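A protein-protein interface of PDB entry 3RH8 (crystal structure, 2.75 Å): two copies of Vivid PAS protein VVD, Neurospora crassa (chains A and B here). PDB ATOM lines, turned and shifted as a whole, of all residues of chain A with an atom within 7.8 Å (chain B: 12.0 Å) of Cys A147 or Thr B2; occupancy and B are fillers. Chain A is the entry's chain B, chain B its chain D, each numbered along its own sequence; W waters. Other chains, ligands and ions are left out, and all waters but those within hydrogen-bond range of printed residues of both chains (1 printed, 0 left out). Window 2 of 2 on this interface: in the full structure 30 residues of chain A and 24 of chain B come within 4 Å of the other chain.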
ATOM      1  N   PRO A  30     -14.121  38.249 -23.715  1.00  0.00           N
ATOM      2  CA  PRO A  30     -12.985  37.881 -22.864  1.00  0.00           C
ATOM      3  C   PRO A  30     -12.772  36.380 -22.649  1.00  0.00           C
ATOM      4  O   PRO A  30     -13.666  35.669 -22.180  1.00  0.00           O
ATOM      5  CB  PRO A  30     -13.298  38.607 -21.558  1.00  0.00           C
ATOM      6  CG  PRO A  30     -14.784  38.463 -21.471  1.00  0.00           C
ATOM      7  CD  PRO A  30     -15.230  38.785 -22.900  1.00  0.00           C
ATOM      8  N   CYS A  35     -10.926  29.193 -19.239  1.00  0.00           N
ATOM      9  CA  CYS A  35     -12.021  29.007 -20.173  1.00  0.00           C
ATOM     10  C   CYS A  35     -12.125  27.559 -20.666  1.00  0.00           C
ATOM     11  O   CYS A  35     -11.110  26.920 -20.954  1.00  0.00           O
ATOM     12  CB  CYS A  35     -11.816  29.945 -21.358  1.00  0.00           C
ATOM     13  SG  CYS A  35     -13.088  29.862 -22.587  1.00  0.00           S
ATOM     14  N   ALA A  36     -13.353  27.047 -20.754  1.00  0.00           N
ATOM     15  CA  ALA A  36     -13.581  25.685 -21.242  1.00  0.00           C
ATOM     16  C   ALA A  36     -13.350  25.686 -22.744  1.00  0.00           C
ATOM     17  O   ALA A  36     -14.200  26.119 -23.530  1.00  0.00           O
ATOM     18  CB  ALA A  36     -15.009  25.222 -20.935  1.00  0.00           C
ATOM     19  N   LEU A  37     -12.188  25.197 -23.142  1.00  0.00           N
ATOM     20  CA  LEU A  37     -11.852  25.173 -24.545  1.00  0.00           C
ATOM     21  C   LEU A  37     -11.169  23.888 -24.966  1.00  0.00           C
ATOM     22  O   LEU A  37     -10.595  23.168 -24.152  1.00  0.00           O
ATOM     23  CB  LEU A  37     -10.962  26.374 -24.873  1.00  0.00           C
ATOM     24  CG  LEU A  37      -9.657  26.515 -24.086  1.00  0.00           C
ATOM     25  CD1 LEU A  37      -8.623  25.510 -24.579  1.00  0.00           C
ATOM     26  CD2 LEU A  37      -9.135  27.924 -24.258  1.00  0.00           C
ATOM     27  N   PHE A  56     -13.230  22.413 -19.610  1.00  0.00           N
ATOM     28  CA  PHE A  56     -14.074  21.677 -20.524  1.00  0.00           C
ATOM     29  C   PHE A  56     -14.391  20.285 -19.968  1.00  0.00           C
ATOM     30  O   PHE A  56     -15.537  19.867 -19.942  1.00  0.00           O
ATOM     31  CB  PHE A  56     -13.375  21.556 -21.874  1.00  0.00           C
ATOM     32  CG  PHE A  56     -14.112  20.704 -22.857  1.00  0.00           C
ATOM     33  CD1 PHE A  56     -15.255  21.179 -23.488  1.00  0.00           C
ATOM     34  CD2 PHE A  56     -13.679  19.412 -23.135  1.00  0.00           C
ATOM     35  CE1 PHE A  56     -15.954  20.379 -24.378  1.00  0.00           C
ATOM     36  CE2 PHE A  56     -14.373  18.605 -24.023  1.00  0.00           C
ATOM     37  CZ  PHE A  56     -15.510  19.087 -24.644  1.00  0.00           C
ATOM     38  N   MET A  59     -16.708  20.564 -16.984  1.00  0.00           N
ATOM     39  CA  MET A  59     -18.031  20.905 -17.477  1.00  0.00           C
ATOM     40  C   MET A  59     -18.781  19.706 -18.049  1.00  0.00           C
ATOM     41  O   MET A  59     -19.870  19.355 -17.583  1.00  0.00           O
ATOM     42  CB  MET A  59     -17.916  21.977 -18.562  1.00  0.00           C
ATOM     43  CG  MET A  59     -19.231  22.360 -19.221  1.00  0.00           C
ATOM     44  SD  MET A  59     -19.029  23.605 -20.519  1.00  0.00           S
ATOM     45  CE  MET A  59     -19.032  22.569 -21.953  1.00  0.00           C
ATOM     46  N   VAL A 111     -22.921  29.719 -31.968  1.00  0.00           N
ATOM     47  CA  VAL A 111     -24.312  29.327 -31.786  1.00  0.00           C
ATOM     48  C   VAL A 111     -24.591  28.871 -30.361  1.00  0.00           C
ATOM     49  O   VAL A 111     -23.699  28.833 -29.522  1.00  0.00           O
ATOM     50  CB  VAL A 111     -24.700  28.142 -32.736  1.00  0.00           C
ATOM     51  CG1 VAL A 111     -24.367  28.473 -34.180  1.00  0.00           C
ATOM     52  CG2 VAL A 111     -23.984  26.881 -32.315  1.00  0.00           C
ATOM     53  N   GLU A 112     -25.854  28.562 -30.092  1.00  0.00           N
ATOM     54  CA  GLU A 112     -26.263  27.998 -28.805  1.00  0.00           C
ATOM     55  C   GLU A 112     -26.641  26.587 -29.214  1.00  0.00           C
ATOM     56  O   GLU A 112     -27.399  26.398 -30.168  1.00  0.00           O
ATOM     57  CB  GLU A 112     -27.507  28.662 -28.235  1.00  0.00           C
ATOM     58  CG  GLU A 112     -27.260  29.864 -27.370  1.00  0.00           C
ATOM     59  CD  GLU A 112     -28.433  30.137 -26.451  1.00  0.00           C
ATOM     60  OE1 GLU A 112     -29.594  29.957 -26.880  1.00  0.00           O
ATOM     61  OE2 GLU A 112     -28.194  30.537 -25.296  1.00  0.00           O
ATOM     62  N   VAL A 113     -26.117  25.596 -28.516  1.00  0.00           N
ATOM     63  CA  VAL A 113     -26.439  24.236 -28.884  1.00  0.00           C
ATOM     64  C   VAL A 113     -26.725  23.378 -27.650  1.00  0.00           C
ATOM     65  O   VAL A 113     -26.177  23.604 -26.566  1.00  0.00           O
ATOM     66  CB  VAL A 113     -25.293  23.648 -29.748  1.00  0.00           C
ATOM     67  CG1 VAL A 113     -24.027  23.590 -28.946  1.00  0.00           C
ATOM     68  CG2 VAL A 113     -25.678  22.282 -30.301  1.00  0.00           C
ATOM     69  N   ASN A 115     -26.248  20.349 -25.478  1.00  0.00           N
ATOM     70  CA  ASN A 115     -25.231  19.337 -25.231  1.00  0.00           C
ATOM     71  C   ASN A 115     -25.622  18.515 -24.008  1.00  0.00           C
ATOM     72  O   ASN A 115     -26.564  18.852 -23.291  1.00  0.00           O
ATOM     73  CB  ASN A 115     -23.846  19.994 -25.043  1.00  0.00           C
ATOM     74  CG  ASN A 115     -23.172  20.396 -26.380  1.00  0.00           C
ATOM     75  OD1 ASN A 115     -22.093  20.998 -26.389  1.00  0.00           O
ATOM     76  ND2 ASN A 115     -23.803  20.049 -27.500  1.00  0.00           N
ATOM     77  N   PHE A 123     -27.800  20.531 -21.261  1.00  0.00           N
ATOM     78  CA  PHE A 123     -27.473  21.918 -20.994  1.00  0.00           C
ATOM     79  C   PHE A 123     -27.264  22.694 -22.291  1.00  0.00           C
ATOM     80  O   PHE A 123     -27.051  22.115 -23.360  1.00  0.00           O
ATOM     81  CB  PHE A 123     -26.232  22.022 -20.117  1.00  0.00           C
ATOM     82  CG  PHE A 123     -24.965  21.635 -20.812  1.00  0.00           C
ATOM     83  CD1 PHE A 123     -24.589  20.303 -20.913  1.00  0.00           C
ATOM     84  CD2 PHE A 123     -24.133  22.615 -21.354  1.00  0.00           C
ATOM     85  CE1 PHE A 123     -23.408  19.948 -21.542  1.00  0.00           C
ATOM     86  CE2 PHE A 123     -22.948  22.266 -21.988  1.00  0.00           C
ATOM     87  CZ  PHE A 123     -22.582  20.931 -22.079  1.00  0.00           C
ATOM     88  N   VAL A 124     -27.356  24.015 -22.195  1.00  0.00           N
ATOM     89  CA  VAL A 124     -27.158  24.859 -23.363  1.00  0.00           C
ATOM     90  C   VAL A 124     -25.695  25.247 -23.397  1.00  0.00           C
ATOM     91  O   VAL A 124     -25.124  25.697 -22.403  1.00  0.00           O
ATOM     92  CB  VAL A 124     -28.022  26.138 -23.313  1.00  0.00           C
ATOM     93  CG1 VAL A 124     -27.772  26.976 -24.544  1.00  0.00           C
ATOM     94  CG2 VAL A 124     -29.494  25.766 -23.254  1.00  0.00           C
ATOM     95  N   ASN A 125     -25.082  25.042 -24.550  1.00  0.00           N
ATOM     96  CA  ASN A 125     -23.685  25.359 -24.716  1.00  0.00           C
ATOM     97  C   ASN A 125     -23.560  26.558 -25.649  1.00  0.00           C
ATOM     98  O   ASN A 125     -23.934  26.481 -26.824  1.00  0.00           O
ATOM     99  CB  ASN A 125     -22.957  24.144 -25.300  1.00  0.00           C
ATOM    100  CG  ASN A 125     -21.459  24.339 -25.374  1.00  0.00           C
ATOM    101  OD1 ASN A 125     -20.983  25.358 -25.846  1.00  0.00           O
ATOM    102  ND2 ASN A 125     -20.708  23.348 -24.914  1.00  0.00           N
ATOM    103  N   PHE A 126     -23.071  27.673 -25.113  1.00  0.00           N
ATOM    104  CA  PHE A 126     -22.851  28.866 -25.921  1.00  0.00           C
ATOM    105  C   PHE A 126     -21.498  28.661 -26.599  1.00  0.00           C
ATOM    106  O   PHE A 126     -20.469  29.122 -26.115  1.00  0.00           O
ATOM    107  CB  PHE A 126     -22.801  30.116 -25.054  1.00  0.00           C
ATOM    108  CG  PHE A 126     -22.533  31.369 -25.832  1.00  0.00           C
ATOM    109  CD1 PHE A 126     -21.511  32.238 -25.455  1.00  0.00           C
ATOM    110  CD2 PHE A 126     -23.279  31.667 -26.967  1.00  0.00           C
ATOM    111  CE1 PHE A 126     -21.238  33.384 -26.198  1.00  0.00           C
ATOM    112  CE2 PHE A 126     -23.012  32.810 -27.715  1.00  0.00           C
ATOM    113  CZ  PHE A 126     -21.991  33.669 -27.334  1.00  0.00           C
ATOM    114  N   LEU A 127     -21.517  27.968 -27.731  1.00  0.00           N
ATOM    115  CA  LEU A 127     -20.299  27.631 -28.456  1.00  0.00           C
ATOM    116  C   LEU A 127     -19.827  28.628 -29.517  1.00  0.00           C
ATOM    117  O   LEU A 127     -20.605  29.393 -30.067  1.00  0.00           O
ATOM    118  CB  LEU A 127     -20.481  26.237 -29.077  1.00  0.00           C
ATOM    119  CG  LEU A 127     -19.352  25.601 -29.892  1.00  0.00           C
ATOM    120  CD1 LEU A 127     -18.161  25.239 -29.016  1.00  0.00           C
ATOM    121  CD2 LEU A 127     -19.907  24.380 -30.565  1.00  0.00           C
ATOM    122  N   THR A 128     -18.527  28.605 -29.784  1.00  0.00           N
ATOM    123  CA  THR A 128     -17.877  29.463 -30.773  1.00  0.00           C
ATOM    124  C   THR A 128     -16.640  28.691 -31.213  1.00  0.00           C
ATOM    125  O   THR A 128     -15.867  28.225 -30.380  1.00  0.00           O
ATOM    126  CB  THR A 128     -17.414  30.845 -30.163  1.00  0.00           C
ATOM    127  OG1 THR A 128     -18.550  31.690 -29.947  1.00  0.00           O
ATOM    128  CG2 THR A 128     -16.444  31.570 -31.091  1.00  0.00           C
ATOM    129  N   GLY A 144     -12.064  25.405 -29.803  1.00  0.00           N
ATOM    130  CA  GLY A 144     -13.439  25.374 -29.342  1.00  0.00           C
ATOM    131  C   GLY A 144     -13.633  26.167 -28.064  1.00  0.00           C
ATOM    132  O   GLY A 144     -12.850  26.034 -27.129  1.00  0.00           O
ATOM    133  N   PHE A 145     -14.674  26.998 -28.032  1.00  0.00           N
ATOM    134  CA  PHE A 145     -15.004  27.834 -26.869  1.00  0.00           C
ATOM    135  C   PHE A 145     -16.377  27.444 -26.318  1.00  0.00           C
ATOM    136  O   PHE A 145     -17.405  27.919 -26.809  1.00  0.00           O
ATOM    137  CB  PHE A 145     -15.053  29.306 -27.272  1.00  0.00           C
ATOM    138  CG  PHE A 145     -13.729  29.881 -27.645  1.00  0.00           C
ATOM    139  CD1 PHE A 145     -12.852  30.306 -26.665  1.00  0.00           C
ATOM    140  CD2 PHE A 145     -13.369  30.017 -28.979  1.00  0.00           C
ATOM    141  CE1 PHE A 145     -11.634  30.866 -27.009  1.00  0.00           C
ATOM    142  CE2 PHE A 145     -12.158  30.574 -29.334  1.00  0.00           C
ATOM    143  CZ  PHE A 145     -11.286  31.002 -28.354  1.00  0.00           C
ATOM    144  N   GLN A 146     -16.402  26.594 -25.296  1.00  0.00           N
ATOM    145  CA  GLN A 146     -17.668  26.165 -24.730  1.00  0.00           C
ATOM    146  C   GLN A 146     -17.998  26.926 -23.452  1.00  0.00           C
ATOM    147  O   GLN A 146     -17.107  27.319 -22.712  1.00  0.00           O
ATOM    148  CB  GLN A 146     -17.632  24.658 -24.465  1.00  0.00           C
ATOM    149  CG  GLN A 146     -17.390  23.797 -25.699  1.00  0.00           C
ATOM    150  CD  GLN A 146     -15.979  23.910 -26.245  1.00  0.00           C
ATOM    151  OE1 GLN A 146     -15.672  23.381 -27.312  1.00  0.00           O
ATOM    152  NE2 GLN A 146     -15.111  24.594 -25.514  1.00  0.00           N
ATOM    153  N   CYS A 147     -19.284  27.147 -23.212  1.00  0.00           N
ATOM    154  CA  CYS A 147     -19.761  27.850 -22.028  1.00  0.00           C
ATOM    155  C   CYS A 147     -21.197  27.432 -21.733  1.00  0.00           C
ATOM    156  O   CYS A 147     -22.036  27.457 -22.643  1.00  0.00           O
ATOM    157  CB  CYS A 147     -19.708  29.376 -22.238  1.00  0.00           C
ATOM    158  SG  CYS A 147     -20.635  30.339 -20.992  1.00  0.00           S
ATOM    159  N   GLU A 148     -21.441  27.039 -20.474  1.00  0.00           N
ATOM    160  CA  GLU A 148     -22.783  26.690 -20.043  1.00  0.00           C
ATOM    161  C   GLU A 148     -23.582  28.071 -19.751  1.00  0.00           C
ATOM    162  O   GLU A 148     -23.937  29.001 -20.223  1.00  0.00           O
ATOM    163  CB  GLU A 148     -22.723  25.637 -18.859  1.00  0.00           C
ATOM    164  CG  GLU A 148     -24.038  24.899 -18.676  1.00  0.00           C
ATOM    165  CD  GLU A 148     -23.949  23.867 -17.569  1.00  0.00           C
ATOM    166  OE1 GLU A 148     -22.979  23.080 -17.568  1.00  0.00           O
ATOM    167  OE2 GLU A 148     -24.847  23.836 -16.705  1.00  0.00           O
ATOM    168  OXT GLU A 148     -23.266  29.041 -18.910  1.00  0.00           O
ATOM    169  N   HIS B   1     -16.496  32.392 -13.237  1.00  0.00           N
ATOM    170  CA  HIS B   1     -16.652  32.684 -14.662  1.00  0.00           C
ATOM    171  C   HIS B   1     -18.106  32.607 -15.140  1.00  0.00           C
ATOM    172  O   HIS B   1     -18.929  31.868 -14.581  1.00  0.00           O
ATOM    173  CB  HIS B   1     -15.773  31.741 -15.508  1.00  0.00           C
ATOM    174  CG  HIS B   1     -15.871  30.293 -15.123  1.00  0.00           C
ATOM    175  ND1 HIS B   1     -15.446  29.812 -13.899  1.00  0.00           N
ATOM    176  CD2 HIS B   1     -16.336  29.218 -15.804  1.00  0.00           C
ATOM    177  CE1 HIS B   1     -15.647  28.509 -13.845  1.00  0.00           C
ATOM    178  NE2 HIS B   1     -16.186  28.122 -14.988  1.00  0.00           N
ATOM    179  N   THR B   2     -18.415  33.383 -16.174  1.00  0.00           N
ATOM    180  CA  THR B   2     -19.761  33.415 -16.735  1.00  0.00           C
ATOM    181  C   THR B   2     -19.721  33.252 -18.264  1.00  0.00           C
ATOM    182  O   THR B   2     -20.080  32.189 -18.785  1.00  0.00           O
ATOM    183  CB  THR B   2     -20.496  34.732 -16.328  1.00  0.00           C
ATOM    184  OG1 THR B   2     -21.690  34.885 -17.105  1.00  0.00           O
ATOM    185  CG2 THR B   2     -19.589  35.945 -16.510  1.00  0.00           C
ATOM    186  N   LEU B   3     -19.283  34.296 -18.974  1.00  0.00           N
ATOM    187  CA  LEU B   3     -19.171  34.256 -20.439  1.00  0.00           C
ATOM    188  C   LEU B   3     -18.031  33.291 -20.779  1.00  0.00           C
ATOM    189  O   LEU B   3     -18.257  32.100 -21.028  1.00  0.00           O
ATOM    190  CB  LEU B   3     -18.857  35.655 -20.995  1.00  0.00           C
ATOM    191  CG  LEU B   3     -19.905  36.339 -21.887  1.00  0.00           C
ATOM    192  CD1 LEU B   3     -21.243  36.472 -21.148  1.00  0.00           C
ATOM    193  CD2 LEU B   3     -19.379  37.709 -22.310  1.00  0.00           C
ATOM    194  N   TYR B   4     -16.805  33.807 -20.790  1.00  0.00           N
ATOM    195  CA  TYR B   4     -15.639  32.976 -21.063  1.00  0.00           C
ATOM    196  C   TYR B   4     -14.514  33.331 -20.089  1.00  0.00           C
ATOM    197  O   TYR B   4     -13.762  32.452 -19.666  1.00  0.00           O
ATOM    198  CB  TYR B   4     -15.156  33.143 -22.514  1.00  0.00           C
ATOM    199  CG  TYR B   4     -16.053  32.524 -23.582  1.00  0.00           C
ATOM    200  CD1 TYR B   4     -16.457  31.184 -23.510  1.00  0.00           C
ATOM    201  CD2 TYR B   4     -16.466  33.274 -24.691  1.00  0.00           C
ATOM    202  CE1 TYR B   4     -17.246  30.610 -24.524  1.00  0.00           C
ATOM    203  CE2 TYR B   4     -17.254  32.711 -25.707  1.00  0.00           C
ATOM    204  CZ  TYR B   4     -17.636  31.383 -25.620  1.00  0.00           C
ATOM    205  OH  TYR B   4     -18.396  30.842 -26.634  1.00  0.00           O
ATOM    206  N   ALA B   5     -14.413  34.611 -19.718  1.00  0.00           N
ATOM    207  CA  ALA B   5     -13.365  35.057 -18.792  1.00  0.00           C
ATOM    208  C   ALA B   5     -13.365  36.565 -18.493  1.00  0.00           C
ATOM    209  O   ALA B   5     -12.480  37.295 -18.962  1.00  0.00           O
ATOM    210  CB  ALA B   5     -12.013  34.661 -19.345  1.00  0.00           C
ATOM    211  N   PRO B   6     -14.340  37.053 -17.702  1.00  0.00           N
ATOM    212  CA  PRO B   6     -14.367  38.491 -17.397  1.00  0.00           C
ATOM    213  C   PRO B   6     -13.611  38.926 -16.138  1.00  0.00           C
ATOM    214  O   PRO B   6     -12.467  39.380 -16.213  1.00  0.00           O
ATOM    215  CB  PRO B   6     -15.856  38.784 -17.298  1.00  0.00           C
ATOM    216  CG  PRO B   6     -16.371  37.534 -16.629  1.00  0.00           C
ATOM    217  CD  PRO B   6     -15.629  36.418 -17.358  1.00  0.00           C
ATOM    218  N   GLY B   7     -14.268  38.785 -14.988  1.00  0.00           N
ATOM    219  CA  GLY B   7     -13.690  39.185 -13.709  1.00  0.00           C
ATOM    220  C   GLY B   7     -12.186  39.057 -13.466  1.00  0.00           C
ATOM    221  O   GLY B   7     -11.689  37.977 -13.093  1.00  0.00           O
ATOM    222  N   GLY B   8     -11.453  40.154 -13.657  1.00  0.00           N
ATOM    223  CA  GLY B   8     -10.023  40.106 -13.413  1.00  0.00           C
ATOM    224  C   GLY B   8      -9.171  41.028 -14.259  1.00  0.00           C
ATOM    225  O   GLY B   8      -9.673  41.761 -15.111  1.00  0.00           O
ATOM    226  N   GLU B  54      -6.328  29.459 -11.566  1.00  0.00           N
ATOM    227  CA  GLU B  54      -6.747  28.262 -10.837  1.00  0.00           C
ATOM    228  C   GLU B  54      -5.670  27.177 -10.840  1.00  0.00           C
ATOM    229  O   GLU B  54      -5.562  26.417  -9.877  1.00  0.00           O
ATOM    230  CB  GLU B  54      -8.036  27.698 -11.430  1.00  0.00           C
ATOM    231  CG  GLU B  54      -9.264  28.526 -11.141  1.00  0.00           C
ATOM    232  CD  GLU B  54     -10.464  28.070 -11.949  1.00  0.00           C
ATOM    233  OE1 GLU B  54     -10.883  26.898 -11.792  1.00  0.00           O
ATOM    234  OE2 GLU B  54     -10.981  28.889 -12.746  1.00  0.00           O
HETATM  235  O   HOH W   1     -16.366  35.979 -22.996  1.00  0.00           O
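Of the printed residues of chain B, Pro A30 touches Tyr B4 and Ala B5.
No residue of chain B comes within 4 Å of Ala A36.
Phe A123 touches none of the printed residues of chain B.
No residue of chain B comes within 4 Å of Val A124.
Of chain B, only Tyr B4 comes within 4 Å of Phe A126.
Leu A127 touches just one residue of chain B: Tyr B4 (3.9 Å).
Of the printed residues of chain B, Phe A145 touches Tyr B4 (3.1 Å).
Of the printed residues of chain B, Gln A146 touches Tyr B4.
Printed residues of chain B within 4 Å of Cys A147: Thr B2 (2.9 Å), Leu B3 (3.0 Å) and Tyr B4 (3.6 Å).
No residue of chain B comes within 4 Å of Glu A148.
Of chain A, only Cys A147 comes within 4 Å of Thr B2.
Of the printed residues of chain A, Leu B3 touches Cys A147.
Of the printed residues of chain A, Tyr B4 touches Pro A30, Cys A35, Phe A126, Leu A127, Thr A128, Phe A145, Gln A146 and Cys A147.
The nearest printed residue of chain B that does not touch Cys A35 is Ala B5 (5.1 Å).
Of the 9 printed residues of chain B, 4 touch a printed residue of chain A.
Hydrophobic or aromatic side chains of chain B within 4 Å of the printed part of chain A: Tyr B4 and Ala B5.
Of the 21 printed residues of chain A, 8 touch a printed residue of chain B.
Printed residues of chain A that touch a printed residue of chain B: Pro A30, Cys A35, Phe A126, Leu A127, Thr A128, Phe A145, Gln A146 and Cys A147.
Along chain A the printed residues that touch a printed residue of chain B span positions 30 to 147.
Among the printed residues, 11 pairs touch across the chains.
O of Phe A126 sits at hydrogen-bond distance from OH of Tyr B4 (2.7 Å).
OH of Tyr B4 is in hydrogen-bond range of OG1 of Thr A128 (3.4 Å).
O of Pro A30 sits at hydrogen-bond distance from N of Ala B5.
OH of Tyr B4 sits at hydrogen-bond distance from O of Phe A145 (3.1 Å).
O of Thr B2 is in hydrogen-bond range of SG of Cys A147, 2.9 Å away.
The side-chain sulfur of Cys A147 is in hydrogen-bond range of the backbone carbonyl oxygen of Leu B3, at 3.0 Å.
O of Pro A30 touches CB of Tyr B4, at 3.0 Å.
O of Tyr B4 touches CB of Cys A35, at 3.6 Å.
Leu A127 touches Tyr B4 (C to OH, 3.9 Å).
Gln A146 touches Tyr B4 (O to CE1, 3.8 Å).
CB of Cys A147 touches CE1 of Tyr B4, 3.6 Å away.
The backbone NH (N) of Phe A126 is in hydrogen-bond range of the backbone carbonyl oxygen (O) of Cys A147, at 2.7 Å.
The backbone carbonyl oxygen (O) of Ala A36 is in hydrogen-bond range of the side-chain amide nitrogen (NE2) of Gln A146 (2.7 Å).
O of Val A111 sits at hydrogen-bond distance from N of Leu A127.
N of Leu A127 sits close to OD1 of Asn A125 (3.3 Å).
The backbone carbonyl oxygen (O) of Gly A144 is in hydrogen-bond range of the side-chain amide nitrogen (NE2) of Gln A146.
The backbone carbonyl oxygen (O) of Thr A128 sits at hydrogen-bond distance from the backbone NH (N) of Phe A145 (2.9 Å).
Water W1 bridges O of Pro A30 (2.8 Å) and N of Tyr B4 (3.1 Å).
No position is printed for both chains.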
